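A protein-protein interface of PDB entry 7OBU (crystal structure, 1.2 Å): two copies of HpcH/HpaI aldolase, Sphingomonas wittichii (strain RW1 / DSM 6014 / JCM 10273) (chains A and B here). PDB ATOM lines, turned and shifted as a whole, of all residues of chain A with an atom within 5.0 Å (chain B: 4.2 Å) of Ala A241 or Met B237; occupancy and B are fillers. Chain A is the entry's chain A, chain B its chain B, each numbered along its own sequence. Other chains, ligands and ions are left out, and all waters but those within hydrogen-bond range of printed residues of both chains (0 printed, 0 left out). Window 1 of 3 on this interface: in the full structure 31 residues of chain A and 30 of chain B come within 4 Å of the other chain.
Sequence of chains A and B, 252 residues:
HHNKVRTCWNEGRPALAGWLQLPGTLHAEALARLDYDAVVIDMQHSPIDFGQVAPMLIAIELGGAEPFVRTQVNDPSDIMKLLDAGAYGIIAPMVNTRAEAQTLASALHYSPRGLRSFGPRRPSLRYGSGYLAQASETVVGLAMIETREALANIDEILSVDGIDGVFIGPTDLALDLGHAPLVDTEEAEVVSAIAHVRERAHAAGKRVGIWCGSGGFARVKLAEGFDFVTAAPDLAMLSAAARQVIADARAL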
ATOM      1  N   ALA A 236       8.797   4.722  -9.579  1.00  0.00           N
ATOM      2  CA  ALA A 236       7.736   5.416 -10.304  1.00  0.00           C
ATOM      3  C   ALA A 236       7.023   4.477 -11.259  1.00  0.00           C
ATOM      4  O   ALA A 236       5.793   4.516 -11.376  1.00  0.00           O
ATOM      5  CB  ALA A 236       8.292   6.618 -11.069  1.00  0.00           C
ATOM      6  N   MET A 237       7.778   3.645 -11.977  1.00  0.00           N
ATOM      7  CA  MET A 237       7.142   2.733 -12.913  1.00  0.00           C
ATOM      8  C   MET A 237       6.278   1.722 -12.168  1.00  0.00           C
ATOM      9  O   MET A 237       5.172   1.386 -12.616  1.00  0.00           O
ATOM     10  CB  MET A 237       8.177   1.987 -13.750  1.00  0.00           C
ATOM     11  CG  MET A 237       8.966   2.856 -14.726  1.00  0.00           C
ATOM     12  SD  MET A 237       9.962   1.907 -15.904  1.00  0.00           S
ATOM     13  CE  MET A 237      11.075   1.068 -14.795  1.00  0.00           C
ATOM     14  N   LEU A 238       6.787   1.203 -11.049  1.00  0.00           N
ATOM     15  CA  LEU A 238       6.058   0.216 -10.264  1.00  0.00           C
ATOM     16  C   LEU A 238       4.802   0.827  -9.639  1.00  0.00           C
ATOM     17  O   LEU A 238       3.737   0.205  -9.641  1.00  0.00           O
ATOM     18  CB  LEU A 238       6.974  -0.330  -9.161  1.00  0.00           C
ATOM     19  CG  LEU A 238       6.331  -1.286  -8.158  1.00  0.00           C
ATOM     20  CD1 LEU A 238       5.636  -2.474  -8.752  1.00  0.00           C
ATOM     21  CD2 LEU A 238       7.415  -1.763  -7.153  1.00  0.00           C
ATOM     22  N   SER A 239       4.918   2.016  -9.062  1.00  0.00           N
ATOM     23  CA  SER A 239       3.749   2.626  -8.446  1.00  0.00           C
ATOM     24  C   SER A 239       2.673   2.904  -9.486  1.00  0.00           C
ATOM     25  O   SER A 239       1.499   2.632  -9.238  1.00  0.00           O
ATOM     26  CB  SER A 239       4.142   3.892  -7.697  1.00  0.00           C
ATOM     27  OG  SER A 239       3.019   4.540  -7.147  1.00  0.00           O
ATOM     28  N   ALA A 240       3.056   3.406 -10.656  1.00  0.00           N
ATOM     29  CA  ALA A 240       2.073   3.682 -11.692  1.00  0.00           C
ATOM     30  C   ALA A 240       1.435   2.397 -12.183  1.00  0.00           C
ATOM     31  O   ALA A 240       0.228   2.349 -12.429  1.00  0.00           O
ATOM     32  CB  ALA A 240       2.718   4.454 -12.835  1.00  0.00           C
ATOM     33  N   ALA A 241       2.228   1.335 -12.302  1.00  0.00           N
ATOM     34  CA  ALA A 241       1.684   0.052 -12.731  1.00  0.00           C
ATOM     35  C   ALA A 241       0.663  -0.470 -11.728  1.00  0.00           C
ATOM     36  O   ALA A 241      -0.420  -0.948 -12.103  1.00  0.00           O
ATOM     37  CB  ALA A 241       2.824  -0.946 -12.932  1.00  0.00           C
ATOM     38  N   ALA A 242       1.000  -0.400 -10.445  1.00  0.00           N
ATOM     39  CA  ALA A 242       0.092  -0.875  -9.420  1.00  0.00           C
ATOM     40  C   ALA A 242      -1.186  -0.063  -9.400  1.00  0.00           C
ATOM     41  O   ALA A 242      -2.271  -0.625  -9.236  1.00  0.00           O
ATOM     42  CB  ALA A 242       0.791  -0.809  -8.065  1.00  0.00           C
ATOM     43  N   ARG A 243      -1.073   1.258  -9.535  1.00  0.00           N
ATOM     44  CA  ARG A 243      -2.271   2.097  -9.558  1.00  0.00           C
ATOM     45  C   ARG A 243      -3.204   1.665 -10.683  1.00  0.00           C
ATOM     46  O   ARG A 243      -4.431   1.616 -10.508  1.00  0.00           O
ATOM     47  CB  ARG A 243      -1.859   3.566  -9.698  1.00  0.00           C
ATOM     48  CG  ARG A 243      -3.022   4.524  -9.744  1.00  0.00           C
ATOM     49  CD  ARG A 243      -2.534   5.930 -10.039  1.00  0.00           C
ATOM     50  NE  ARG A 243      -1.462   6.322  -9.129  1.00  0.00           N
ATOM     51  CZ  ARG A 243      -1.647   6.839  -7.920  1.00  0.00           C
ATOM     52  NH1 ARG A 243      -2.861   7.024  -7.421  1.00  0.00           N
ATOM     53  NH2 ARG A 243      -0.588   7.181  -7.191  1.00  0.00           N
ATOM     54  N   GLN A 244      -2.637   1.362 -11.849  1.00  0.00           N
ATOM     55  CA  GLN A 244      -3.448   0.948 -12.993  1.00  0.00           C
ATOM     56  C   GLN A 244      -4.047  -0.442 -12.788  1.00  0.00           C
ATOM     57  O   GLN A 244      -5.190  -0.684 -13.177  1.00  0.00           O
ATOM     58  CB  GLN A 244      -2.640   0.995 -14.290  1.00  0.00           C
ATOM     59  CG  GLN A 244      -3.490   0.742 -15.533  1.00  0.00           C
ATOM     60  CD  GLN A 244      -4.530   1.822 -15.748  1.00  0.00           C
ATOM     61  OE1 GLN A 244      -4.199   3.004 -15.905  1.00  0.00           O
ATOM     62  NE2 GLN A 244      -5.792   1.433 -15.722  1.00  0.00           N
ATOM     63  N   VAL A 245      -3.281  -1.374 -12.200  1.00  0.00           N
ATOM     64  CA  VAL A 245      -3.834  -2.690 -11.875  1.00  0.00           C
ATOM     65  C   VAL A 245      -5.023  -2.545 -10.937  1.00  0.00           C
ATOM     66  O   VAL A 245      -6.061  -3.192 -11.128  1.00  0.00           O
ATOM     67  CB  VAL A 245      -2.749  -3.609 -11.290  1.00  0.00           C
ATOM     68  CG1 VAL A 245      -3.387  -4.811 -10.595  1.00  0.00           C
ATOM     69  CG2 VAL A 245      -1.798  -4.065 -12.369  1.00  0.00           C
ATOM     70  N   ALA B 232      -0.986  -7.181  -8.709  1.00  0.00           N
ATOM     71  CA  ALA B 232      -0.284  -8.305  -9.311  1.00  0.00           C
ATOM     72  C   ALA B 232       1.148  -8.216  -8.725  1.00  0.00           C
ATOM     73  O   ALA B 232       1.504  -7.232  -8.105  1.00  0.00           O
ATOM     74  CB  ALA B 232      -0.273  -8.178 -10.830  1.00  0.00           C
ATOM     75  N   PRO B 233       1.976  -9.235  -8.898  1.00  0.00           N
ATOM     76  CA  PRO B 233       3.293  -9.190  -8.248  1.00  0.00           C
ATOM     77  C   PRO B 233       4.108  -7.973  -8.659  1.00  0.00           C
ATOM     78  O   PRO B 233       4.199  -7.642  -9.846  1.00  0.00           O
ATOM     79  CB  PRO B 233       3.960 -10.492  -8.707  1.00  0.00           C
ATOM     80  CG  PRO B 233       2.833 -11.406  -8.977  1.00  0.00           C
ATOM     81  CD  PRO B 233       1.751 -10.535  -9.552  1.00  0.00           C
ATOM     82  N   ASP B 234       4.752  -7.355  -7.660  1.00  0.00           N
ATOM     83  CA  ASP B 234       5.601  -6.192  -7.917  1.00  0.00           C
ATOM     84  C   ASP B 234       6.617  -6.440  -9.026  1.00  0.00           C
ATOM     85  O   ASP B 234       6.751  -5.620  -9.939  1.00  0.00           O
ATOM     86  CB  ASP B 234       6.276  -5.678  -6.634  1.00  0.00           C
ATOM     87  CG  ASP B 234       7.101  -6.729  -5.848  1.00  0.00           C
ATOM     88  OD1 ASP B 234       7.190  -7.906  -6.246  1.00  0.00           O
ATOM     89  OD2 ASP B 234       7.626  -6.323  -4.779  1.00  0.00           O
ATOM     90  N   LEU B 235       7.363  -7.537  -8.961  1.00  0.00           N
ATOM     91  CA  LEU B 235       8.401  -7.750  -9.962  1.00  0.00           C
ATOM     92  C   LEU B 235       7.817  -7.852 -11.364  1.00  0.00           C
ATOM     93  O   LEU B 235       8.376  -7.305 -12.317  1.00  0.00           O
ATOM     94  CB  LEU B 235       9.173  -9.020  -9.629  1.00  0.00           C
ATOM     95  CG  LEU B 235      10.220  -9.470 -10.646  1.00  0.00           C
ATOM     96  CD1 LEU B 235      11.286  -8.433 -10.892  1.00  0.00           C
ATOM     97  CD2 LEU B 235      10.832 -10.818 -10.220  1.00  0.00           C
ATOM     98  N   ALA B 236       6.713  -8.585 -11.516  1.00  0.00           N
ATOM     99  CA  ALA B 236       6.077  -8.722 -12.826  1.00  0.00           C
ATOM    100  C   ALA B 236       5.544  -7.386 -13.340  1.00  0.00           C
ATOM    101  O   ALA B 236       5.735  -7.052 -14.522  1.00  0.00           O
ATOM    102  CB  ALA B 236       4.980  -9.776 -12.742  1.00  0.00           C
ATOM    103  N   MET B 237       4.924  -6.586 -12.462  1.00  0.00           N
ATOM    104  CA  MET B 237       4.442  -5.275 -12.872  1.00  0.00           C
ATOM    105  C   MET B 237       5.584  -4.363 -13.276  1.00  0.00           C
ATOM    106  O   MET B 237       5.508  -3.656 -14.292  1.00  0.00           O
ATOM    107  CB  MET B 237       3.632  -4.607 -11.769  1.00  0.00           C
ATOM    108  CG  MET B 237       2.336  -5.315 -11.456  1.00  0.00           C
ATOM    109  SD  MET B 237       1.221  -4.380 -10.360  1.00  0.00           S
ATOM    110  CE  MET B 237       2.286  -4.186  -8.937  1.00  0.00           C
ATOM    111  N   LEU B 238       6.676  -4.395 -12.513  1.00  0.00           N
ATOM    112  CA  LEU B 238       7.811  -3.530 -12.802  1.00  0.00           C
ATOM    113  C   LEU B 238       8.498  -3.946 -14.100  1.00  0.00           C
ATOM    114  O   LEU B 238       8.857  -3.091 -14.917  1.00  0.00           O
ATOM    115  CB  LEU B 238       8.794  -3.636 -11.635  1.00  0.00           C
ATOM    116  CG  LEU B 238      10.139  -2.952 -11.816  1.00  0.00           C
ATOM    117  CD1 LEU B 238      10.016  -1.484 -12.130  1.00  0.00           C
ATOM    118  CD2 LEU B 238      10.974  -3.162 -10.578  1.00  0.00           C
ATOM    119  N   SER B 239       8.707  -5.247 -14.304  1.00  0.00           N
ATOM    120  CA  SER B 239       9.351  -5.732 -15.521  1.00  0.00           C
ATOM    121  C   SER B 239       8.544  -5.356 -16.749  1.00  0.00           C
ATOM    122  O   SER B 239       9.089  -4.904 -17.762  1.00  0.00           O
ATOM    123  CB  SER B 239       9.452  -7.250 -15.453  1.00  0.00           C
ATOM    124  OG  SER B 239      10.323  -7.627 -14.414  1.00  0.00           O
ATOM    125  N   ALA B 240       7.224  -5.548 -16.672  1.00  0.00           N
ATOM    126  CA  ALA B 240       6.366  -5.199 -17.801  1.00  0.00           C
ATOM    127  C   ALA B 240       6.421  -3.697 -18.069  1.00  0.00           C
ATOM    128  O   ALA B 240       6.482  -3.257 -19.232  1.00  0.00           O
ATOM    129  CB  ALA B 240       4.936  -5.676 -17.559  1.00  0.00           C
ATOM    130  N   ALA B 241       6.420  -2.894 -17.007  1.00  0.00           N
ATOM    131  CA  ALA B 241       6.495  -1.447 -17.179  1.00  0.00           C
ATOM    132  C   ALA B 241       7.799  -1.046 -17.851  1.00  0.00           C
ATOM    133  O   ALA B 241       7.808  -0.200 -18.761  1.00  0.00           O
ATOM    134  CB  ALA B 241       6.317  -0.744 -15.835  1.00  0.00           C
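Of the 10 printed residues of chain B, 5 touch a printed residue of chain A.
Printed residues of chain B that touch a printed residue of chain A: Ala B232, Asp B234, Met B237, Leu B238 and Ala B241.
Along chain B the printed residues that touch a printed residue of chain A span positions 232 to 241.
Of the 10 printed residues of chain A, 5 touch a printed residue of chain B.
Printed residues of chain A that touch a printed residue of chain B: Met A237, Leu A238, Ala A241, Ala A242 and Val A245.
Among the printed residues, 8 pairs touch across the chains.
Among the printed residues, no Asp or Glu carboxylate lies within 4 Å of a Lys or Arg side-chain nitrogen of the other chain.
Printed residues of chain B within 4 Å of Met A237: Leu B238 and Ala B241.
Of chain B, only Met B237 (3.9 Å) comes within 4 Å of Ala A241.
Of the printed residues of chain B, Ala A242 touches Met B237 (3.8 Å).
Of the printed residues of chain B, Val A245 touches Ala B232 and Met B237.
Met B237 touches four residues of chain A.
Printed residues of chain A within 4 Å of Leu B238: Met A237 (3.8 Å).
Ala B240 touches none of the printed residues of chain A.
The nearest printed residue of chain B that does not touch Ala A241 is Ala B241 (4.5 Å).
The nearest printed residue of chain A that does not touch Ala B232 is Leu A238 (6.3 Å).
Met A237 touches Leu B238 (CE to CD1, 3.8 Å).
CB of Met A237 touches CB of Ala B241 (3.9 Å).
CD1 of Leu A238 touches O of Asp B234 (3.5 Å).
Met B237 touches Leu A238 (CE to CD1, 3.8 Å).
CB of Ala A241 touches CB of Met B237 (3.9 Å).
Met B237 touches Ala A242.
Val A245 touches Ala B232 (CG1 to N, 3.9 Å).
SD of Met B237 touches CG2 of Val A245 (3.6 Å).
Met A237 touches Leu B238, and with the chains exchanged Leu A238 touches Met B237.
Met A237 touches Ala B241, and with the chains exchanged Ala A241 touches Met B237.
Positions printed for both chains: 236, 237, 238, 239, 240 and 241.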
